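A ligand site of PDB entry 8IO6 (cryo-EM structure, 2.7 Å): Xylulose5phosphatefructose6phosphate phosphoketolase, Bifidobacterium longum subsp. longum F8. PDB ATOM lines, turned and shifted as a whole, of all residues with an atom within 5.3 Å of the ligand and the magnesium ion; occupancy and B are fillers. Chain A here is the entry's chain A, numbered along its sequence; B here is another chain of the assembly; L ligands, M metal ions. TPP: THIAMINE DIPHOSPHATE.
The side-chain hydroxyl of Thr 187 lies within hydrogen-bond range of the backbone carbonyl oxygen of Glu 184 (2.4 Å).
ND2 of Asn 215 sits at hydrogen-bond distance from O of Gly 66 (3.3 Å).
A ring nitrogen (ND1) of His 320 sits at hydrogen-bond distance from the side-chain amino group (NZ) of Lys 300 (3.3 Å).
N of Asp 182 sits at hydrogen-bond distance from O of His 213, 3.5 Å away.
N of Ile 219 is in hydrogen-bond range of OD2 of Asp 436 of chain B (2.9 Å).
The backbone NH (N) of Gly 216 sits at hydrogen-bond distance from the side-chain carboxylate (OD2) of Asp 182, 2.6 Å away.
O of Lys 218 is in hydrogen-bond range of NZ of Lys 300 (3.2 Å).
The side-chain amide nitrogen (ND2) of Asn 215 lies within hydrogen-bond range of a ring nitrogen (NE2) of His 213.
The backbone NH (N) of Glu 184 sits at hydrogen-bond distance from an oxygen (O1A) of the ligand, 2.9 Å away.
The backbone NH (N) of Gly 183 lies within hydrogen-bond range of an oxygen (O1A) of the ligand (3.4 Å).
The side-chain amino group (NZ) of Lys 300 lies within salt-bridge range of an oxygen (O3B) of the ligand.
The side-chain hydroxyl (OG1) of Thr 67 lies close to an oxygen (O1B) of the ligand (3.2 Å).
The backbone carbonyl oxygen (O) of Gly 155 is in hydrogen-bond range of a nitrogen (N4') of the ligand (2.6 Å).
The backbone NH (N) of Leu 157 is in hydrogen-bond range of a nitrogen (N3') of the ligand (3.3 Å).
An oxygen (O3B) of the ligand is in hydrogen-bond range of a ring nitrogen (NE2) of His 97 (3.0 Å).
Three residues have an atom within 4 Å of the magnesium ion: Asp 182, Asn 215 and Tyr 217.
The nearest printed residue that does not touch the magnesium ion is Lys 300 (4.1 Å).
The magnesium ion is bound by an oxygen (O2B) of the ligand (1.9 Å), the side-chain amide oxygen of Asn 215 (2.0 Å), the side-chain carboxylate of Asp 182 (2.0 Å), the backbone carbonyl oxygen of Tyr 217 (2.2 Å) and an oxygen (O2A) of the ligand (2.5 Å).
The magnesium ion has five donor atoms within binding distance.
N1' of the ligand sits close to OE2 of Glu 479 of chain B (3.0 Å).
CB of Pro 95 touches O1B of the ligand (3.9 Å).
Glu 156 touches the ligand.
Gly 181 touches the ligand.
His 213 touches the ligand.
CD1 of Ile 219 touches C4 of the ligand, 3.5 Å away.
His 320 touches the ligand.
Asp 436 of chain B touches the ligand (OD2 to CM4, 3.6 Å).
Glu 437 of chain B touches the ligand (OE2 to C6', 3.3 Å).
Leu 477 of chain B touches the ligand (CD1 to CM4, 3.5 Å).
Phe 504 of chain B touches the ligand (CE2 to C5', 3.3 Å).
His 553 of chain B touches the ligand (NE2 to N4', 3.6 Å).
Hydrophobic or aromatic side chains within 4 Å of the ligand: Pro 95, His 97, Leu 157, His 213, Ile 219, His 320, Leu 477 of chain B and Phe 504 of chain B.
Of the 32 residues printed, 22 come within 4 Å of the ligand.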
ATOM      1  N   GLY A  66      30.631   9.749 -22.331  1.00  0.00           N
ATOM      2  CA  GLY A  66      31.063  11.133 -22.460  1.00  0.00           C
ATOM      3  C   GLY A  66      31.635  11.712 -21.183  1.00  0.00           C
ATOM      4  O   GLY A  66      32.269  12.764 -21.193  1.00  0.00           O
ATOM      5  N   THR A  67      31.424  11.030 -20.053  1.00  0.00           N
ATOM      6  CA  THR A  67      31.981  11.491 -18.797  1.00  0.00           C
ATOM      7  C   THR A  67      32.920  10.473 -18.163  1.00  0.00           C
ATOM      8  O   THR A  67      33.648  10.834 -17.242  1.00  0.00           O
ATOM      9  CB  THR A  67      30.854  11.824 -17.813  1.00  0.00           C
ATOM     10  OG1 THR A  67      31.411  12.371 -16.619  1.00  0.00           O
ATOM     11  CG2 THR A  67      30.050  10.601 -17.479  1.00  0.00           C
ATOM     12  N   PRO A  95      27.441  13.335 -12.071  1.00  0.00           N
ATOM     13  CA  PRO A  95      26.975  12.641 -13.277  1.00  0.00           C
ATOM     14  C   PRO A  95      26.974  11.133 -13.086  1.00  0.00           C
ATOM     15  O   PRO A  95      27.944  10.455 -13.424  1.00  0.00           O
ATOM     16  CB  PRO A  95      27.971  13.086 -14.347  1.00  0.00           C
ATOM     17  CG  PRO A  95      28.672  14.267 -13.777  1.00  0.00           C
ATOM     18  CD  PRO A  95      28.702  14.032 -12.309  1.00  0.00           C
ATOM     19  N   HIS A  97      25.489   8.839 -14.564  1.00  0.00           N
ATOM     20  CA  HIS A  97      25.465   8.014 -15.757  1.00  0.00           C
ATOM     21  C   HIS A  97      26.850   7.540 -16.139  1.00  0.00           C
ATOM     22  O   HIS A  97      26.996   6.643 -16.974  1.00  0.00           O
ATOM     23  CB  HIS A  97      24.826   8.779 -16.915  1.00  0.00           C
ATOM     24  CG  HIS A  97      25.355  10.161 -17.108  1.00  0.00           C
ATOM     25  ND1 HIS A  97      24.896  11.237 -16.382  1.00  0.00           N
ATOM     26  CD2 HIS A  97      26.317  10.645 -17.926  1.00  0.00           C
ATOM     27  CE1 HIS A  97      25.546  12.320 -16.754  1.00  0.00           C
ATOM     28  NE2 HIS A  97      26.414  11.987 -17.688  1.00  0.00           N
ATOM     29  N   GLY A 154      22.730   9.532  -8.752  1.00  0.00           N
ATOM     30  CA  GLY A 154      23.113  10.435  -9.812  1.00  0.00           C
ATOM     31  C   GLY A 154      22.260  10.353 -11.056  1.00  0.00           C
ATOM     32  O   GLY A 154      22.558  11.063 -12.025  1.00  0.00           O
ATOM     33  N   GLY A 155      21.244   9.504 -11.072  1.00  0.00           N
ATOM     34  CA  GLY A 155      20.404   9.410 -12.258  1.00  0.00           C
ATOM     35  C   GLY A 155      19.626  10.683 -12.527  1.00  0.00           C
ATOM     36  O   GLY A 155      19.589  11.177 -13.658  1.00  0.00           O
ATOM     37  N   GLU A 156      19.007  11.223 -11.488  1.00  0.00           N
ATOM     38  CA  GLU A 156      18.245  12.454 -11.606  1.00  0.00           C
ATOM     39  C   GLU A 156      19.095  13.576 -11.012  1.00  0.00           C
ATOM     40  O   GLU A 156      19.523  13.490  -9.861  1.00  0.00           O
ATOM     41  CB  GLU A 156      16.894  12.265 -10.919  1.00  0.00           C
ATOM     42  CG  GLU A 156      15.886  13.343 -11.125  1.00  0.00           C
ATOM     43  CD  GLU A 156      16.105  14.429 -10.148  1.00  0.00           C
ATOM     44  OE1 GLU A 156      16.613  14.081  -9.066  1.00  0.00           O
ATOM     45  OE2 GLU A 156      15.786  15.596 -10.421  1.00  0.00           O
ATOM     46  N   LEU A 157      19.333  14.608 -11.825  1.00  0.00           N
ATOM     47  CA  LEU A 157      20.471  15.502 -11.615  1.00  0.00           C
ATOM     48  C   LEU A 157      20.108  16.715 -10.770  1.00  0.00           C
ATOM     49  O   LEU A 157      18.978  17.203 -10.788  1.00  0.00           O
ATOM     50  CB  LEU A 157      21.005  15.982 -12.968  1.00  0.00           C
ATOM     51  CG  LEU A 157      21.607  14.981 -13.941  1.00  0.00           C
ATOM     52  CD1 LEU A 157      22.115  15.705 -15.168  1.00  0.00           C
ATOM     53  CD2 LEU A 157      22.722  14.197 -13.294  1.00  0.00           C
ATOM     54  N   GLY A 181      28.690  17.710 -12.847  1.00  0.00           N
ATOM     55  CA  GLY A 181      28.646  17.885 -14.276  1.00  0.00           C
ATOM     56  C   GLY A 181      28.309  19.315 -14.651  1.00  0.00           C
ATOM     57  O   GLY A 181      27.590  20.012 -13.940  1.00  0.00           O
ATOM     58  N   ASP A 182      28.835  19.763 -15.782  1.00  0.00           N
ATOM     59  CA  ASP A 182      28.611  21.141 -16.182  1.00  0.00           C
ATOM     60  C   ASP A 182      27.204  21.337 -16.710  1.00  0.00           C
ATOM     61  O   ASP A 182      26.644  22.435 -16.601  1.00  0.00           O
ATOM     62  CB  ASP A 182      29.649  21.570 -17.230  1.00  0.00           C
ATOM     63  CG  ASP A 182      29.705  20.655 -18.425  1.00  0.00           C
ATOM     64  OD1 ASP A 182      29.115  19.562 -18.392  1.00  0.00           O
ATOM     65  OD2 ASP A 182      30.347  21.038 -19.411  1.00  0.00           O
ATOM     66  N   GLY A 183      26.616  20.298 -17.297  1.00  0.00           N
ATOM     67  CA  GLY A 183      25.208  20.362 -17.640  1.00  0.00           C
ATOM     68  C   GLY A 183      24.316  20.319 -16.412  1.00  0.00           C
ATOM     69  O   GLY A 183      23.349  21.075 -16.314  1.00  0.00           O
ATOM     70  N   GLU A 184      24.648  19.434 -15.464  1.00  0.00           N
ATOM     71  CA  GLU A 184      23.920  19.358 -14.214  1.00  0.00           C
ATOM     72  C   GLU A 184      23.972  20.670 -13.442  1.00  0.00           C
ATOM     73  O   GLU A 184      23.039  21.003 -12.707  1.00  0.00           O
ATOM     74  CB  GLU A 184      24.486  18.219 -13.378  1.00  0.00           C
ATOM     75  CG  GLU A 184      24.203  18.285 -11.899  1.00  0.00           C
ATOM     76  CD  GLU A 184      24.967  17.223 -11.133  1.00  0.00           C
ATOM     77  OE1 GLU A 184      26.030  16.793 -11.608  1.00  0.00           O
ATOM     78  OE2 GLU A 184      24.484  16.807 -10.061  1.00  0.00           O
ATOM     79  N   ALA A 185      25.032  21.451 -13.635  1.00  0.00           N
ATOM     80  CA  ALA A 185      25.142  22.739 -12.969  1.00  0.00           C
ATOM     81  C   ALA A 185      24.108  23.727 -13.473  1.00  0.00           C
ATOM     82  O   ALA A 185      23.915  24.779 -12.860  1.00  0.00           O
ATOM     83  CB  ALA A 185      26.546  23.297 -13.149  1.00  0.00           C
ATOM     84  N   THR A 187      20.920  22.873 -13.701  1.00  0.00           N
ATOM     85  CA  THR A 187      19.687  22.548 -13.013  1.00  0.00           C
ATOM     86  C   THR A 187      19.491  23.466 -11.810  1.00  0.00           C
ATOM     87  O   THR A 187      20.439  23.947 -11.203  1.00  0.00           O
ATOM     88  CB  THR A 187      19.685  21.093 -12.563  1.00  0.00           C
ATOM     89  OG1 THR A 187      20.809  20.842 -11.718  1.00  0.00           O
ATOM     90  CG2 THR A 187      19.748  20.171 -13.758  1.00  0.00           C
ATOM     91  N   HIS A 213      33.062  19.298 -13.341  1.00  0.00           N
ATOM     92  CA  HIS A 213      33.536  18.469 -14.452  1.00  0.00           C
ATOM     93  C   HIS A 213      33.038  19.095 -15.744  1.00  0.00           C
ATOM     94  O   HIS A 213      32.063  18.669 -16.355  1.00  0.00           O
ATOM     95  CB  HIS A 213      33.056  17.036 -14.263  1.00  0.00           C
ATOM     96  CG  HIS A 213      33.367  16.137 -15.411  1.00  0.00           C
ATOM     97  ND1 HIS A 213      34.641  15.942 -15.889  1.00  0.00           N
ATOM     98  CD2 HIS A 213      32.567  15.306 -16.124  1.00  0.00           C
ATOM     99  CE1 HIS A 213      34.616  15.076 -16.888  1.00  0.00           C
ATOM    100  NE2 HIS A 213      33.367  14.675 -17.037  1.00  0.00           N
ATOM    101  N   ASN A 215      33.231  19.487 -19.116  1.00  0.00           N
ATOM    102  CA  ASN A 215      33.627  18.957 -20.409  1.00  0.00           C
ATOM    103  C   ASN A 215      32.890  19.617 -21.574  1.00  0.00           C
ATOM    104  O   ASN A 215      33.089  19.207 -22.718  1.00  0.00           O
ATOM    105  CB  ASN A 215      33.457  17.438 -20.457  1.00  0.00           C
ATOM    106  CG  ASN A 215      32.079  16.966 -20.063  1.00  0.00           C
ATOM    107  OD1 ASN A 215      31.123  17.725 -20.064  1.00  0.00           O
ATOM    108  ND2 ASN A 215      31.971  15.701 -19.739  1.00  0.00           N
ATOM    109  N   GLY A 216      32.077  20.624 -21.308  1.00  0.00           N
ATOM    110  CA  GLY A 216      31.544  21.482 -22.339  1.00  0.00           C
ATOM    111  C   GLY A 216      30.188  21.150 -22.897  1.00  0.00           C
ATOM    112  O   GLY A 216      29.549  22.000 -23.508  1.00  0.00           O
ATOM    113  N   TYR A 217      29.730  19.915 -22.707  1.00  0.00           N
ATOM    114  CA  TYR A 217      28.549  19.435 -23.390  1.00  0.00           C
ATOM    115  C   TYR A 217      27.619  18.661 -22.462  1.00  0.00           C
ATOM    116  O   TYR A 217      28.048  17.969 -21.541  1.00  0.00           O
ATOM    117  CB  TYR A 217      28.927  18.562 -24.583  1.00  0.00           C
ATOM    118  CG  TYR A 217      29.856  19.269 -25.521  1.00  0.00           C
ATOM    119  CD1 TYR A 217      29.379  20.153 -26.469  1.00  0.00           C
ATOM    120  CD2 TYR A 217      31.223  19.079 -25.439  1.00  0.00           C
ATOM    121  CE1 TYR A 217      30.226  20.813 -27.304  1.00  0.00           C
ATOM    122  CE2 TYR A 217      32.063  19.735 -26.267  1.00  0.00           C
ATOM    123  CZ  TYR A 217      31.577  20.599 -27.192  1.00  0.00           C
ATOM    124  OH  TYR A 217      32.446  21.252 -28.027  1.00  0.00           O
ATOM    125  N   LYS A 218      26.332  18.840 -22.735  1.00  0.00           N
ATOM    126  CA  LYS A 218      25.225  18.024 -22.270  1.00  0.00           C
ATOM    127  C   LYS A 218      24.966  16.917 -23.287  1.00  0.00           C
ATOM    128  O   LYS A 218      25.865  16.568 -24.057  1.00  0.00           O
ATOM    129  CB  LYS A 218      23.976  18.879 -22.084  1.00  0.00           C
ATOM    130  CG  LYS A 218      24.194  20.062 -21.192  1.00  0.00           C
ATOM    131  CD  LYS A 218      22.893  20.754 -20.874  1.00  0.00           C
ATOM    132  CE  LYS A 218      22.328  21.527 -22.041  1.00  0.00           C
ATOM    133  NZ  LYS A 218      23.068  22.780 -22.284  1.00  0.00           N
ATOM    134  N   ILE A 219      23.783  16.321 -23.276  1.00  0.00           N
ATOM    135  CA  ILE A 219      23.301  15.529 -24.397  1.00  0.00           C
ATOM    136  C   ILE A 219      23.008  16.499 -25.529  1.00  0.00           C
ATOM    137  O   ILE A 219      22.100  17.329 -25.414  1.00  0.00           O
ATOM    138  CB  ILE A 219      22.024  14.736 -24.047  1.00  0.00           C
ATOM    139  CG1 ILE A 219      22.238  13.849 -22.835  1.00  0.00           C
ATOM    140  CG2 ILE A 219      21.609  13.879 -25.221  1.00  0.00           C
ATOM    141  CD1 ILE A 219      20.956  13.255 -22.327  1.00  0.00           C
ATOM    142  N   THR A 223      27.032  23.411 -22.726  1.00  0.00           N
ATOM    143  CA  THR A 223      26.637  23.929 -21.425  1.00  0.00           C
ATOM    144  C   THR A 223      26.914  25.420 -21.340  1.00  0.00           C
ATOM    145  O   THR A 223      27.859  25.929 -21.940  1.00  0.00           O
ATOM    146  CB  THR A 223      27.373  23.187 -20.319  1.00  0.00           C
ATOM    147  OG1 THR A 223      28.764  23.511 -20.363  1.00  0.00           O
ATOM    148  CG2 THR A 223      27.221  21.714 -20.505  1.00  0.00           C
ATOM    149  N   LYS A 300      35.039  16.010 -23.740  1.00  0.00           N
ATOM    150  CA  LYS A 300      34.080  14.939 -23.508  1.00  0.00           C
ATOM    151  C   LYS A 300      34.475  13.682 -24.257  1.00  0.00           C
ATOM    152  O   LYS A 300      34.755  13.720 -25.452  1.00  0.00           O
ATOM    153  CB  LYS A 300      32.697  15.418 -23.934  1.00  0.00           C
ATOM    154  CG  LYS A 300      31.574  14.479 -23.589  1.00  0.00           C
ATOM    155  CD  LYS A 300      30.273  15.227 -23.417  1.00  0.00           C
ATOM    156  CE  LYS A 300      29.208  14.320 -22.876  1.00  0.00           C
ATOM    157  NZ  LYS A 300      28.078  15.088 -22.323  1.00  0.00           N
ATOM    158  N   HIS A 320      28.439  11.312 -25.955  1.00  0.00           N
ATOM    159  CA  HIS A 320      27.718  11.218 -24.683  1.00  0.00           C
ATOM    160  C   HIS A 320      27.391   9.777 -24.331  1.00  0.00           C
ATOM    161  O   HIS A 320      27.940   9.222 -23.370  1.00  0.00           O
ATOM    162  CB  HIS A 320      26.444  12.051 -24.743  1.00  0.00           C
ATOM    163  CG  HIS A 320      25.597  11.941 -23.519  1.00  0.00           C
ATOM    164  ND1 HIS A 320      25.936  12.545 -22.320  1.00  0.00           N
ATOM    165  CD2 HIS A 320      24.431  11.295 -23.292  1.00  0.00           C
ATOM    166  CE1 HIS A 320      25.013  12.277 -21.425  1.00  0.00           C
ATOM    167  NE2 HIS A 320      24.095  11.515 -21.972  1.00  0.00           N
ATOM    168  N   PRO B 435      14.254  20.413 -21.915  1.00  0.00           N
ATOM    169  CA  PRO B 435      15.408  20.345 -21.004  1.00  0.00           C
ATOM    170  C   PRO B 435      16.517  19.447 -21.534  1.00  0.00           C
ATOM    171  O   PRO B 435      16.816  18.382 -20.991  1.00  0.00           O
ATOM    172  CB  PRO B 435      14.773  19.793 -19.724  1.00  0.00           C
ATOM    173  CG  PRO B 435      13.615  19.008 -20.189  1.00  0.00           C
ATOM    174  CD  PRO B 435      13.070  19.733 -21.367  1.00  0.00           C
ATOM    175  N   ASP B 436      17.148  19.904 -22.624  1.00  0.00           N
ATOM    176  CA  ASP B 436      18.260  19.219 -23.281  1.00  0.00           C
ATOM    177  C   ASP B 436      17.830  17.952 -23.996  1.00  0.00           C
ATOM    178  O   ASP B 436      18.656  17.083 -24.299  1.00  0.00           O
ATOM    179  CB  ASP B 436      19.382  18.938 -22.278  1.00  0.00           C
ATOM    180  CG  ASP B 436      20.645  18.439 -22.926  1.00  0.00           C
ATOM    181  OD1 ASP B 436      21.169  19.158 -23.806  1.00  0.00           O
ATOM    182  OD2 ASP B 436      21.123  17.341 -22.567  1.00  0.00           O
ATOM    183  N   GLU B 437      16.544  17.820 -24.326  1.00  0.00           N
ATOM    184  CA  GLU B 437      15.996  16.540 -24.742  1.00  0.00           C
ATOM    185  C   GLU B 437      15.150  16.617 -26.017  1.00  0.00           C
ATOM    186  O   GLU B 437      14.432  15.657 -26.318  1.00  0.00           O
ATOM    187  CB  GLU B 437      15.171  15.968 -23.587  1.00  0.00           C
ATOM    188  CG  GLU B 437      16.046  15.589 -22.398  1.00  0.00           C
ATOM    189  CD  GLU B 437      15.271  15.057 -21.239  1.00  0.00           C
ATOM    190  OE1 GLU B 437      14.018  15.096 -21.304  1.00  0.00           O
ATOM    191  OE2 GLU B 437      15.889  14.598 -20.270  1.00  0.00           O
ATOM    192  N   LEU B 477      19.240  22.743 -19.606  1.00  0.00           N
ATOM    193  CA  LEU B 477      19.068  21.574 -18.749  1.00  0.00           C
ATOM    194  C   LEU B 477      18.489  21.997 -17.405  1.00  0.00           C
ATOM    195  O   LEU B 477      19.155  22.057 -16.379  1.00  0.00           O
ATOM    196  CB  LEU B 477      20.384  20.833 -18.581  1.00  0.00           C
ATOM    197  CG  LEU B 477      20.335  19.556 -17.732  1.00  0.00           C
ATOM    198  CD1 LEU B 477      19.121  18.746 -18.089  1.00  0.00           C
ATOM    199  CD2 LEU B 477      21.586  18.765 -17.951  1.00  0.00           C
ATOM    200  N   GLU B 479      14.235  21.719 -15.984  1.00  0.00           N
ATOM    201  CA  GLU B 479      12.796  21.635 -16.253  1.00  0.00           C
ATOM    202  C   GLU B 479      12.066  22.852 -15.718  1.00  0.00           C
ATOM    203  O   GLU B 479      11.071  23.287 -16.314  1.00  0.00           O
ATOM    204  CB  GLU B 479      12.200  20.364 -15.670  1.00  0.00           C
ATOM    205  CG  GLU B 479      12.846  19.042 -16.133  1.00  0.00           C
ATOM    206  CD  GLU B 479      14.266  18.819 -15.611  1.00  0.00           C
ATOM    207  OE1 GLU B 479      14.461  18.858 -14.374  1.00  0.00           O
ATOM    208  OE2 GLU B 479      15.173  18.601 -16.439  1.00  0.00           O
ATOM    209  N   TYR B 501      11.405  13.881 -20.718  1.00  0.00           N
ATOM    210  CA  TYR B 501      11.358  12.523 -20.183  1.00  0.00           C
ATOM    211  C   TYR B 501      10.218  12.408 -19.190  1.00  0.00           C
ATOM    212  O   TYR B 501       9.888  13.367 -18.485  1.00  0.00           O
ATOM    213  CB  TYR B 501      12.665  12.193 -19.475  1.00  0.00           C
ATOM    214  CG  TYR B 501      13.810  11.766 -20.362  1.00  0.00           C
ATOM    215  CD1 TYR B 501      13.859  12.137 -21.698  1.00  0.00           C
ATOM    216  CD2 TYR B 501      14.863  11.038 -19.854  1.00  0.00           C
ATOM    217  CE1 TYR B 501      14.910  11.767 -22.502  1.00  0.00           C
ATOM    218  CE2 TYR B 501      15.925  10.665 -20.651  1.00  0.00           C
ATOM    219  CZ  TYR B 501      15.939  11.035 -21.972  1.00  0.00           C
ATOM    220  OH  TYR B 501      16.990  10.665 -22.763  1.00  0.00           O
ATOM    221  N   PHE B 504      11.122  12.784 -15.231  1.00  0.00           N
ATOM    222  CA  PHE B 504      11.549  14.075 -14.709  1.00  0.00           C
ATOM    223  C   PHE B 504      10.458  15.134 -14.757  1.00  0.00           C
ATOM    224  O   PHE B 504      10.687  16.249 -14.285  1.00  0.00           O
ATOM    225  CB  PHE B 504      12.789  14.557 -15.457  1.00  0.00           C
ATOM    226  CG  PHE B 504      13.911  13.573 -15.428  1.00  0.00           C
ATOM    227  CD1 PHE B 504      14.252  12.941 -14.255  1.00  0.00           C
ATOM    228  CD2 PHE B 504      14.596  13.247 -16.574  1.00  0.00           C
ATOM    229  CE1 PHE B 504      15.260  12.021 -14.209  1.00  0.00           C
ATOM    230  CE2 PHE B 504      15.610  12.319 -16.527  1.00  0.00           C
ATOM    231  CZ  PHE B 504      15.938  11.715 -15.348  1.00  0.00           C
ATOM    232  N   VAL B 507       9.753  16.843 -11.555  1.00  0.00           N
ATOM    233  CA  VAL B 507      10.522  18.017 -11.140  1.00  0.00           C
ATOM    234  C   VAL B 507       9.634  19.257 -11.131  1.00  0.00           C
ATOM    235  O   VAL B 507       9.840  20.166 -10.327  1.00  0.00           O
ATOM    236  CB  VAL B 507      11.740  18.187 -12.059  1.00  0.00           C
ATOM    237  CG1 VAL B 507      12.398  19.530 -11.854  1.00  0.00           C
ATOM    238  CG2 VAL B 507      12.733  17.073 -11.816  1.00  0.00           C
ATOM    239  N   HIS B 553      15.421   6.361 -14.152  1.00  0.00           N
ATOM    240  CA  HIS B 553      14.684   7.148 -15.127  1.00  0.00           C
ATOM    241  C   HIS B 553      13.286   6.620 -15.388  1.00  0.00           C
ATOM    242  O   HIS B 553      12.686   6.974 -16.413  1.00  0.00           O
ATOM    243  CB  HIS B 553      15.453   7.215 -16.433  1.00  0.00           C
ATOM    244  CG  HIS B 553      16.671   8.088 -16.377  1.00  0.00           C
ATOM    245  ND1 HIS B 553      17.732   7.824 -15.545  1.00  0.00           N
ATOM    246  CD2 HIS B 553      16.992   9.208 -17.055  1.00  0.00           C
ATOM    247  CE1 HIS B 553      18.655   8.754 -15.704  1.00  0.00           C
ATOM    248  NE2 HIS B 553      18.227   9.615 -16.615  1.00  0.00           N
HETATM  249  N1' TPP L   1      16.941  16.170 -16.412  1.00  0.00           N
HETATM  250  C2' TPP L   1      17.297  15.786 -15.177  1.00  0.00           C
HETATM  251  CM2 TPP L   1      16.827  16.633 -14.039  1.00  0.00           C
HETATM  252  N3' TPP L   1      18.055  14.731 -14.872  1.00  0.00           N
HETATM  253  C4' TPP L   1      18.486  13.962 -15.888  1.00  0.00           C
HETATM  254  N4' TPP L   1      19.239  12.904 -15.561  1.00  0.00           N
HETATM  255  C5' TPP L   1      18.163  14.277 -17.231  1.00  0.00           C
HETATM  256  C6' TPP L   1      17.390  15.393 -17.405  1.00  0.00           C
HETATM  257  C7' TPP L   1      18.631  13.452 -18.399  1.00  0.00           C
HETATM  258  N3  TPP L   1      20.098  13.370 -18.510  1.00  0.00           N
HETATM  259  C2  TPP L   1      20.816  12.325 -18.148  1.00  0.00           C
HETATM  260  S1  TPP L   1      22.442  12.556 -18.394  1.00  0.00           S
HETATM  261  C5  TPP L   1      22.168  14.138 -19.020  1.00  0.00           C
HETATM  262  C4  TPP L   1      20.865  14.425 -19.002  1.00  0.00           C
HETATM  263  CM4 TPP L   1      20.214  15.685 -19.470  1.00  0.00           C
HETATM  264  C6  TPP L   1      23.306  15.005 -19.474  1.00  0.00           C
HETATM  265  C7  TPP L   1      24.447  15.048 -18.485  1.00  0.00           C
HETATM  266  O7  TPP L   1      24.923  16.416 -18.400  1.00  0.00           O
HETATM  267  PA  TPP L   1      26.276  16.817 -17.727  1.00  0.00           P
HETATM  268  O1A TPP L   1      26.089  17.087 -16.283  1.00  0.00           O
HETATM  269  O2A TPP L   1      26.946  17.889 -18.538  1.00  0.00           O
HETATM  270  O3A TPP L   1      27.095  15.536 -17.932  1.00  0.00           O
HETATM  271  PB  TPP L   1      28.356  15.039 -18.743  1.00  0.00           P
HETATM  272  O1B TPP L   1      29.296  14.536 -17.696  1.00  0.00           O
HETATM  273  O2B TPP L   1      28.908  16.144 -19.570  1.00  0.00           O
HETATM  274  O3B TPP L   1      27.854  13.877 -19.536  1.00  0.00           O
HETATM  275 MG    MG M   1      29.223  18.016 -19.645  1.00  0.00          MG
